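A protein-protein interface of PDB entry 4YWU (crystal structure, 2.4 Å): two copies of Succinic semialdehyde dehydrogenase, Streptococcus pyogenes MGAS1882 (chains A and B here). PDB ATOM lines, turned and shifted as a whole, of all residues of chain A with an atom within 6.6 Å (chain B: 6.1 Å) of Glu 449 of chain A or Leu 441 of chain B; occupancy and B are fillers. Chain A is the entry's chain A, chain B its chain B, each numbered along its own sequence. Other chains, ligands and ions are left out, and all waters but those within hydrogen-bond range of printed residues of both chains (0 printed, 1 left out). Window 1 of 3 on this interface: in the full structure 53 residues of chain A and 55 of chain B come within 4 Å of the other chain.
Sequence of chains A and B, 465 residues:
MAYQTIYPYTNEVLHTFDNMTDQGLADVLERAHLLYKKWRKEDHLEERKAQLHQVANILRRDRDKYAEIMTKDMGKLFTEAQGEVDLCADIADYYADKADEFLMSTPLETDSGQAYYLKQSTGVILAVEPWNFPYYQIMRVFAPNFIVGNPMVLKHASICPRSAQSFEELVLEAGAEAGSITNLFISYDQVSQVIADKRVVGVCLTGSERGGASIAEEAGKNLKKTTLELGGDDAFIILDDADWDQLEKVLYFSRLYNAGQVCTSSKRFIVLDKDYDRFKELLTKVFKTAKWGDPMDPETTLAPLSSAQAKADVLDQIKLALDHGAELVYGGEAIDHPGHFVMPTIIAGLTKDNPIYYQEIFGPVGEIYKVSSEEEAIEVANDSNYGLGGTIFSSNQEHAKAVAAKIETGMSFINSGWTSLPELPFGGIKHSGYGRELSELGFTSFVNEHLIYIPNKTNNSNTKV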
ATOM      1  N   TYR A 117      13.325  -9.610 -28.738  1.00  0.00           N
ATOM      2  CA  TYR A 117      13.902  -9.050 -27.534  1.00  0.00           C
ATOM      3  C   TYR A 117      15.331  -8.571 -27.747  1.00  0.00           C
ATOM      4  O   TYR A 117      16.111  -9.165 -28.499  1.00  0.00           O
ATOM      5  CB  TYR A 117      13.800 -10.047 -26.368  1.00  0.00           C
ATOM      6  CG  TYR A 117      14.692 -11.263 -26.428  1.00  0.00           C
ATOM      7  CD1 TYR A 117      16.039 -11.182 -26.083  1.00  0.00           C
ATOM      8  CD2 TYR A 117      14.175 -12.511 -26.777  1.00  0.00           C
ATOM      9  CE1 TYR A 117      16.849 -12.314 -26.079  1.00  0.00           C
ATOM     10  CE2 TYR A 117      14.978 -13.647 -26.777  1.00  0.00           C
ATOM     11  CZ  TYR A 117      16.313 -13.539 -26.424  1.00  0.00           C
ATOM     12  OH  TYR A 117      17.113 -14.658 -26.411  1.00  0.00           O
ATOM     13  N   LEU A 118      15.647  -7.462 -27.092  1.00  0.00           N
ATOM     14  CA  LEU A 118      16.962  -6.842 -27.173  1.00  0.00           C
ATOM     15  C   LEU A 118      17.862  -7.359 -26.059  1.00  0.00           C
ATOM     16  O   LEU A 118      17.396  -7.721 -24.976  1.00  0.00           O
ATOM     17  CB  LEU A 118      16.820  -5.328 -27.039  1.00  0.00           C
ATOM     18  CG  LEU A 118      15.809  -4.700 -27.997  1.00  0.00           C
ATOM     19  CD1 LEU A 118      15.601  -3.219 -27.662  1.00  0.00           C
ATOM     20  CD2 LEU A 118      16.315  -4.876 -29.419  1.00  0.00           C
ATOM     21  N   LYS A 119      19.155  -7.405 -26.341  1.00  0.00           N
ATOM     22  CA  LYS A 119      20.130  -7.849 -25.363  1.00  0.00           C
ATOM     23  C   LYS A 119      20.816  -6.576 -24.897  1.00  0.00           C
ATOM     24  O   LYS A 119      21.649  -6.012 -25.608  1.00  0.00           O
ATOM     25  CB  LYS A 119      21.114  -8.822 -26.017  1.00  0.00           C
ATOM     26  CG  LYS A 119      20.432 -10.104 -26.450  1.00  0.00           C
ATOM     27  CD  LYS A 119      21.348 -11.068 -27.176  1.00  0.00           C
ATOM     28  CE  LYS A 119      20.592 -12.362 -27.494  1.00  0.00           C
ATOM     29  NZ  LYS A 119      21.400 -13.328 -28.287  1.00  0.00           N
ATOM     30  N   GLN A 120      20.452  -6.113 -23.707  1.00  0.00           N
ATOM     31  CA  GLN A 120      21.014  -4.876 -23.192  1.00  0.00           C
ATOM     32  C   GLN A 120      21.858  -5.008 -21.935  1.00  0.00           C
ATOM     33  O   GLN A 120      21.748  -5.978 -21.189  1.00  0.00           O
ATOM     34  CB  GLN A 120      19.884  -3.874 -22.939  1.00  0.00           C
ATOM     35  CG  GLN A 120      19.058  -3.577 -24.174  1.00  0.00           C
ATOM     36  CD  GLN A 120      17.871  -2.687 -23.890  1.00  0.00           C
ATOM     37  OE1 GLN A 120      17.141  -2.893 -22.919  1.00  0.00           O
ATOM     38  NE2 GLN A 120      17.658  -1.699 -24.746  1.00  0.00           N
ATOM     39  N   THR A 122      23.146  -4.045 -18.136  1.00  0.00           N
ATOM     40  CA  THR A 122      22.325  -3.864 -16.934  1.00  0.00           C
ATOM     41  C   THR A 122      22.914  -2.957 -15.854  1.00  0.00           C
ATOM     42  O   THR A 122      22.170  -2.345 -15.098  1.00  0.00           O
ATOM     43  CB  THR A 122      21.950  -5.234 -16.298  1.00  0.00           C
ATOM     44  OG1 THR A 122      23.125  -6.040 -16.139  1.00  0.00           O
ATOM     45  CG2 THR A 122      20.952  -5.974 -17.187  1.00  0.00           C
ATOM     46  N   THR A 444      25.381 -13.843 -21.905  1.00  0.00           N
ATOM     47  CA  THR A 444      24.098 -13.321 -21.457  1.00  0.00           C
ATOM     48  C   THR A 444      23.790 -13.456 -19.967  1.00  0.00           C
ATOM     49  O   THR A 444      22.633 -13.311 -19.574  1.00  0.00           O
ATOM     50  CB  THR A 444      22.940 -13.981 -22.234  1.00  0.00           C
ATOM     51  OG1 THR A 444      23.015 -15.403 -22.086  1.00  0.00           O
ATOM     52  CG2 THR A 444      23.017 -13.633 -23.704  1.00  0.00           C
ATOM     53  N   SER A 445      24.798 -13.712 -19.138  1.00  0.00           N
ATOM     54  CA  SER A 445      24.558 -13.869 -17.697  1.00  0.00           C
ATOM     55  C   SER A 445      23.991 -12.633 -17.018  1.00  0.00           C
ATOM     56  O   SER A 445      23.098 -12.735 -16.181  1.00  0.00           O
ATOM     57  CB  SER A 445      25.840 -14.286 -16.965  1.00  0.00           C
ATOM     58  OG  SER A 445      26.095 -15.670 -17.140  1.00  0.00           O
ATOM     59  N   PHE A 446      24.516 -11.468 -17.372  1.00  0.00           N
ATOM     60  CA  PHE A 446      24.054 -10.221 -16.783  1.00  0.00           C
ATOM     61  C   PHE A 446      23.514  -9.307 -17.869  1.00  0.00           C
ATOM     62  O   PHE A 446      23.739  -8.093 -17.874  1.00  0.00           O
ATOM     63  CB  PHE A 446      25.202  -9.563 -16.016  1.00  0.00           C
ATOM     64  CG  PHE A 446      25.689 -10.392 -14.863  1.00  0.00           C
ATOM     65  CD1 PHE A 446      24.931 -10.490 -13.693  1.00  0.00           C
ATOM     66  CD2 PHE A 446      26.858 -11.138 -14.970  1.00  0.00           C
ATOM     67  CE1 PHE A 446      25.330 -11.325 -12.647  1.00  0.00           C
ATOM     68  CE2 PHE A 446      27.268 -11.974 -13.936  1.00  0.00           C
ATOM     69  CZ  PHE A 446      26.499 -12.071 -12.766  1.00  0.00           C
ATOM     70  N   VAL A 447      22.787  -9.922 -18.789  1.00  0.00           N
ATOM     71  CA  VAL A 447      22.185  -9.222 -19.902  1.00  0.00           C
ATOM     72  C   VAL A 447      20.700  -9.073 -19.624  1.00  0.00           C
ATOM     73  O   VAL A 447      20.100  -9.880 -18.906  1.00  0.00           O
ATOM     74  CB  VAL A 447      22.408 -10.006 -21.206  1.00  0.00           C
ATOM     75  CG1 VAL A 447      21.408  -9.588 -22.260  1.00  0.00           C
ATOM     76  CG2 VAL A 447      23.804  -9.758 -21.704  1.00  0.00           C
ATOM     77  N   ASN A 448      20.110  -8.022 -20.179  1.00  0.00           N
ATOM     78  CA  ASN A 448      18.695  -7.769 -19.997  1.00  0.00           C
ATOM     79  C   ASN A 448      17.960  -8.159 -21.265  1.00  0.00           C
ATOM     80  O   ASN A 448      18.140  -7.526 -22.302  1.00  0.00           O
ATOM     81  CB  ASN A 448      18.467  -6.285 -19.692  1.00  0.00           C
ATOM     82  CG  ASN A 448      16.996  -5.897 -19.730  1.00  0.00           C
ATOM     83  OD1 ASN A 448      16.111  -6.753 -19.639  1.00  0.00           O
ATOM     84  ND2 ASN A 448      16.727  -4.600 -19.847  1.00  0.00           N
ATOM     85  N   GLU A 449      17.164  -9.222 -21.207  1.00  0.00           N
ATOM     86  CA  GLU A 449      16.400  -9.619 -22.383  1.00  0.00           C
ATOM     87  C   GLU A 449      15.162  -8.740 -22.356  1.00  0.00           C
ATOM     88  O   GLU A 449      14.193  -9.033 -21.647  1.00  0.00           O
ATOM     89  CB  GLU A 449      15.990 -11.089 -22.326  1.00  0.00           C
ATOM     90  CG  GLU A 449      17.133 -12.093 -22.380  1.00  0.00           C
ATOM     91  CD  GLU A 449      17.897 -12.200 -21.064  1.00  0.00           C
ATOM     92  OE1 GLU A 449      17.272 -12.065 -19.981  1.00  0.00           O
ATOM     93  OE2 GLU A 449      19.126 -12.442 -21.117  1.00  0.00           O
ATOM     94  N   HIS A 450      15.218  -7.653 -23.118  1.00  0.00           N
ATOM     95  CA  HIS A 450      14.136  -6.684 -23.191  1.00  0.00           C
ATOM     96  C   HIS A 450      13.141  -7.008 -24.300  1.00  0.00           C
ATOM     97  O   HIS A 450      13.384  -6.725 -25.464  1.00  0.00           O
ATOM     98  CB  HIS A 450      14.731  -5.293 -23.403  1.00  0.00           C
ATOM     99  CG  HIS A 450      13.742  -4.180 -23.259  1.00  0.00           C
ATOM    100  ND1 HIS A 450      14.123  -2.858 -23.185  1.00  0.00           N
ATOM    101  CD2 HIS A 450      12.390  -4.190 -23.172  1.00  0.00           C
ATOM    102  CE1 HIS A 450      13.048  -2.100 -23.057  1.00  0.00           C
ATOM    103  NE2 HIS A 450      11.983  -2.883 -23.047  1.00  0.00           N
ATOM    104  N   LEU A 451      12.015  -7.599 -23.922  1.00  0.00           N
ATOM    105  CA  LEU A 451      10.980  -7.970 -24.870  1.00  0.00           C
ATOM    106  C   LEU A 451      10.269  -6.755 -25.447  1.00  0.00           C
ATOM    107  O   LEU A 451       9.927  -5.822 -24.723  1.00  0.00           O
ATOM    108  CB  LEU A 451       9.941  -8.861 -24.186  1.00  0.00           C
ATOM    109  CG  LEU A 451       8.667  -9.162 -24.986  1.00  0.00           C
ATOM    110  CD1 LEU A 451       8.956 -10.201 -26.066  1.00  0.00           C
ATOM    111  CD2 LEU A 451       7.596  -9.678 -24.053  1.00  0.00           C
ATOM    112  N   THR B 409      13.780  -1.499 -18.652  1.00  0.00           N
ATOM    113  CA  THR B 409      12.720  -2.377 -18.214  1.00  0.00           C
ATOM    114  C   THR B 409      12.896  -3.719 -18.921  1.00  0.00           C
ATOM    115  O   THR B 409      13.688  -3.831 -19.857  1.00  0.00           O
ATOM    116  CB  THR B 409      11.344  -1.755 -18.553  1.00  0.00           C
ATOM    117  OG1 THR B 409      10.312  -2.472 -17.868  1.00  0.00           O
ATOM    118  CG2 THR B 409      11.081  -1.797 -20.060  1.00  0.00           C
ATOM    119  N   GLY B 410      12.167  -4.732 -18.473  1.00  0.00           N
ATOM    120  CA  GLY B 410      12.292  -6.040 -19.081  1.00  0.00           C
ATOM    121  C   GLY B 410      11.369  -6.291 -20.260  1.00  0.00           C
ATOM    122  O   GLY B 410      11.640  -7.160 -21.092  1.00  0.00           O
ATOM    123  N   MET B 411      10.278  -5.536 -20.346  1.00  0.00           N
ATOM    124  CA  MET B 411       9.325  -5.725 -21.433  1.00  0.00           C
ATOM    125  C   MET B 411       8.677  -4.413 -21.846  1.00  0.00           C
ATOM    126  O   MET B 411       8.487  -3.513 -21.021  1.00  0.00           O
ATOM    127  CB  MET B 411       8.233  -6.698 -20.999  1.00  0.00           C
ATOM    128  CG  MET B 411       8.757  -7.996 -20.417  1.00  0.00           C
ATOM    129  SD  MET B 411       7.475  -8.893 -19.523  1.00  0.00           S
ATOM    130  CE  MET B 411       7.385  -7.945 -18.001  1.00  0.00           C
ATOM    131  N   PRO B 425       8.890 -14.236 -23.343  1.00  0.00           N
ATOM    132  CA  PRO B 425       9.621 -14.223 -22.070  1.00  0.00           C
ATOM    133  C   PRO B 425       9.065 -13.141 -21.140  1.00  0.00           C
ATOM    134  O   PRO B 425       8.667 -12.076 -21.596  1.00  0.00           O
ATOM    135  CB  PRO B 425      11.063 -13.954 -22.501  1.00  0.00           C
ATOM    136  CG  PRO B 425      10.896 -13.155 -23.750  1.00  0.00           C
ATOM    137  CD  PRO B 425       9.790 -13.895 -24.458  1.00  0.00           C
ATOM    138  N   GLY B 427       9.815 -11.118 -17.360  1.00  0.00           N
ATOM    139  CA  GLY B 427      10.663 -10.873 -16.215  1.00  0.00           C
ATOM    140  C   GLY B 427      11.149  -9.450 -16.327  1.00  0.00           C
ATOM    141  O   GLY B 427      10.812  -8.764 -17.293  1.00  0.00           O
ATOM    142  N   GLY B 435      15.893 -12.890 -14.072  1.00  0.00           N
ATOM    143  CA  GLY B 435      15.546 -14.195 -14.594  1.00  0.00           C
ATOM    144  C   GLY B 435      14.274 -14.032 -15.409  1.00  0.00           C
ATOM    145  O   GLY B 435      13.452 -13.159 -15.127  1.00  0.00           O
ATOM    146  N   ARG B 436      14.109 -14.869 -16.424  1.00  0.00           N
ATOM    147  CA  ARG B 436      12.940 -14.790 -17.284  1.00  0.00           C
ATOM    148  C   ARG B 436      12.109 -16.065 -17.251  1.00  0.00           C
ATOM    149  O   ARG B 436      12.651 -17.165 -17.231  1.00  0.00           O
ATOM    150  CB  ARG B 436      13.380 -14.498 -18.721  1.00  0.00           C
ATOM    151  CG  ARG B 436      13.959 -13.118 -18.911  1.00  0.00           C
ATOM    152  CD  ARG B 436      12.881 -12.082 -18.729  1.00  0.00           C
ATOM    153  NE  ARG B 436      13.335 -10.723 -19.005  1.00  0.00           N
ATOM    154  CZ  ARG B 436      14.133 -10.027 -18.206  1.00  0.00           C
ATOM    155  NH1 ARG B 436      14.569 -10.564 -17.075  1.00  0.00           N
ATOM    156  NH2 ARG B 436      14.478  -8.789 -18.535  1.00  0.00           N
ATOM    157  N   GLU B 437      10.790 -15.906 -17.238  1.00  0.00           N
ATOM    158  CA  GLU B 437       9.875 -17.038 -17.229  1.00  0.00           C
ATOM    159  C   GLU B 437       9.108 -17.108 -18.544  1.00  0.00           C
ATOM    160  O   GLU B 437       8.928 -16.097 -19.222  1.00  0.00           O
ATOM    161  CB  GLU B 437       8.934 -16.942 -16.032  1.00  0.00           C
ATOM    162  CG  GLU B 437       9.614 -17.417 -14.751  1.00  0.00           C
ATOM    163  CD  GLU B 437       8.708 -17.398 -13.523  1.00  0.00           C
ATOM    164  OE1 GLU B 437       7.475 -17.574 -13.682  1.00  0.00           O
ATOM    165  OE2 GLU B 437       9.236 -17.232 -12.394  1.00  0.00           O
ATOM    166  N   LEU B 438       8.671 -18.314 -18.902  1.00  0.00           N
ATOM    167  CA  LEU B 438       7.962 -18.556 -20.158  1.00  0.00           C
ATOM    168  C   LEU B 438       8.944 -18.469 -21.322  1.00  0.00           C
ATOM    169  O   LEU B 438      10.093 -18.055 -21.154  1.00  0.00           O
ATOM    170  CB  LEU B 438       6.806 -17.574 -20.339  1.00  0.00           C
ATOM    171  CG  LEU B 438       5.673 -17.822 -19.348  1.00  0.00           C
ATOM    172  CD1 LEU B 438       4.655 -16.705 -19.429  1.00  0.00           C
ATOM    173  CD2 LEU B 438       5.034 -19.181 -19.645  1.00  0.00           C
ATOM    174  N   SER B 439       8.484 -18.854 -22.505  1.00  0.00           N
ATOM    175  CA  SER B 439       9.339 -18.870 -23.685  1.00  0.00           C
ATOM    176  C   SER B 439      10.403 -19.944 -23.455  1.00  0.00           C
ATOM    177  O   SER B 439      10.238 -20.818 -22.603  1.00  0.00           O
ATOM    178  CB  SER B 439      10.010 -17.510 -23.873  1.00  0.00           C
ATOM    179  OG  SER B 439      10.764 -17.488 -25.072  1.00  0.00           O
ATOM    180  N   GLU B 440      11.492 -19.883 -24.213  1.00  0.00           N
ATOM    181  CA  GLU B 440      12.568 -20.853 -24.066  1.00  0.00           C
ATOM    182  C   GLU B 440      13.559 -20.417 -22.997  1.00  0.00           C
ATOM    183  O   GLU B 440      14.250 -21.246 -22.406  1.00  0.00           O
ATOM    184  CB  GLU B 440      13.286 -21.062 -25.397  1.00  0.00           C
ATOM    185  CG  GLU B 440      14.507 -21.962 -25.297  1.00  0.00           C
ATOM    186  CD  GLU B 440      14.863 -22.625 -26.619  1.00  0.00           C
ATOM    187  OE1 GLU B 440      14.859 -21.916 -27.651  1.00  0.00           O
ATOM    188  OE2 GLU B 440      15.154 -23.849 -26.619  1.00  0.00           O
ATOM    189  N   LEU B 441      13.627 -19.116 -22.740  1.00  0.00           N
ATOM    190  CA  LEU B 441      14.535 -18.610 -21.720  1.00  0.00           C
ATOM    191  C   LEU B 441      14.044 -19.080 -20.357  1.00  0.00           C
ATOM    192  O   LEU B 441      14.832 -19.290 -19.435  1.00  0.00           O
ATOM    193  CB  LEU B 441      14.581 -17.081 -21.744  1.00  0.00           C
ATOM    194  CG  LEU B 441      14.775 -16.406 -23.105  1.00  0.00           C
ATOM    195  CD1 LEU B 441      14.971 -14.912 -22.904  1.00  0.00           C
ATOM    196  CD2 LEU B 441      15.980 -17.001 -23.814  1.00  0.00           C
ATOM    197  N   GLY B 442      12.732 -19.248 -20.233  1.00  0.00           N
ATOM    198  CA  GLY B 442      12.163 -19.687 -18.972  1.00  0.00           C
ATOM    199  C   GLY B 442      12.294 -21.183 -18.789  1.00  0.00           C
ATOM    200  O   GLY B 442      12.312 -21.683 -17.661  1.00  0.00           O
ATOM    201  N   PHE B 443      12.399 -21.893 -19.906  1.00  0.00           N
ATOM    202  CA  PHE B 443      12.523 -23.343 -19.897  1.00  0.00           C
ATOM    203  C   PHE B 443      13.849 -23.823 -19.298  1.00  0.00           C
ATOM    204  O   PHE B 443      13.906 -24.857 -18.623  1.00  0.00           O
ATOM    205  CB  PHE B 443      12.401 -23.872 -21.321  1.00  0.00           C
ATOM    206  CG  PHE B 443      12.390 -25.368 -21.413  1.00  0.00           C
ATOM    207  CD1 PHE B 443      11.270 -26.094 -21.016  1.00  0.00           C
ATOM    208  CD2 PHE B 443      13.494 -26.055 -21.912  1.00  0.00           C
ATOM    209  CE1 PHE B 443      11.249 -27.487 -21.121  1.00  0.00           C
ATOM    210  CE2 PHE B 443      13.484 -27.448 -22.020  1.00  0.00           C
ATOM    211  CZ  PHE B 443      12.358 -28.164 -21.625  1.00  0.00           C
ATOM    212  N   THR B 444      14.914 -23.067 -19.531  1.00  0.00           N
ATOM    213  CA  THR B 444      16.225 -23.458 -19.045  1.00  0.00           C
ATOM    214  C   THR B 444      16.668 -22.931 -17.677  1.00  0.00           C
ATOM    215  O   THR B 444      17.761 -23.270 -17.219  1.00  0.00           O
ATOM    216  CB  THR B 444      17.303 -23.096 -20.087  1.00  0.00           C
ATOM    217  OG1 THR B 444      17.271 -21.690 -20.353  1.00  0.00           O
ATOM    218  CG2 THR B 444      17.045 -23.829 -21.375  1.00  0.00           C
ATOM    219  N   SER B 445      15.846 -22.123 -17.016  1.00  0.00           N
ATOM    220  CA  SER B 445      16.232 -21.583 -15.709  1.00  0.00           C
ATOM    221  C   SER B 445      16.861 -22.613 -14.754  1.00  0.00           C
ATOM    222  O   SER B 445      17.851 -22.323 -14.081  1.00  0.00           O
ATOM    223  CB  SER B 445      15.027 -20.936 -15.018  1.00  0.00           C
ATOM    224  OG  SER B 445      14.674 -19.715 -15.636  1.00  0.00           O
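O of Leu 118 of chain A sits at hydrogen-bond distance from N of His 450 of chain A (2.9 Å). O of Gln 120 of chain A is in hydrogen-bond range of N of Asn 448 of chain A. ND1 of His 450 of chain A sits at hydrogen-bond distance from OE1 of Gln 120 of chain A (3.0 Å).
Among the printed residues, pairs that only touch across the chains: Tyr 117 of chain A with Leu 441 of chain B (3.7 Å), Asn 448 of chain A with Gly 410 of chain B (3.9 Å), Glu 449 of chain A with Leu 441 of chain B (3.6 Å), His 450 of chain A with Gly 410 of chain B (3.3 Å), His 450 of chain A with Met 411 of chain B (3.8 Å), Leu 451 of chain A with Met 411 of chain B (3.3 Å) and Leu 451 of chain A with Pro 425 of chain B (3.6 Å).
Positions printed for both chains: 444 and 445. Of the 13 pairs that touch across the chains among the printed residues, none has its exchanged pair printed and touching as well.
Of the printed residues of chain B, Glu 449 of chain A touches Gly 410 (3.2 Å), Arg 436 (3.1 Å) and Leu 441 (3.6 Å). Printed residues of chain A within 4 Å of Thr 409 of chain B: Asn 448 (3.1 Å) and His 450 (3.3 Å). Printed residues of chain A within 4 Å of Gly 410 of chain B: Asn 448 (3.9 Å), Glu 449 (3.2 Å), His 450 (3.3 Å) and Leu 451 (2.9 Å). Printed residues of chain A within 4 Å of Pro 425 of chain B: Leu 451 (3.6 Å). Gly 435 of chain B touches none of the printed residues of chain A. Ser 439 of chain B touches none of the printed residues of chain A. Of chain A, only Tyr 117 and Glu 449 come within 4 Å of Leu 441 of chain B. The nearest printed residue of chain A that does not touch Leu 441 of chain B is His 450 of chain A (7.3 Å). The nearest printed residue of chain B that does not touch His 450 of chain A is Arg 436 of chain B (4.8 Å).
Of the 13 printed residues of chain A, 5 touch a printed residue of chain B. Hydrophobic or aromatic side chains of chain A that line the printed part of chain B: Tyr 117, His 450 and Leu 451. Among the printed residues, 13 pairs touch across the chains.
The side-chain amide nitrogen of Asn 448 of chain A is in hydrogen-bond range of the backbone carbonyl oxygen of Thr 409 of chain B. The side-chain amide oxygen (OD1) of Asn 448 of chain A sits at hydrogen-bond distance from the guanidinium group (NH2) of Arg 436 of chain B. The guanidinium group (NH2) of Arg 436 of chain B lies within hydrogen-bond range of the backbone carbonyl oxygen (O) of Glu 449 of chain A, at 3.1 Å. ND1 of His 450 of chain A sits close to O of Thr 409 of chain B. The backbone carbonyl oxygen of Gly 410 of chain B lies within hydrogen-bond range of the backbone NH of Leu 451 of chain A, at 2.9 Å. The backbone carbonyl oxygen (O) of Gly 410 of chain B sits close to the backbone carbonyl oxygen (O) of Glu 449 of chain A (3.2 Å).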
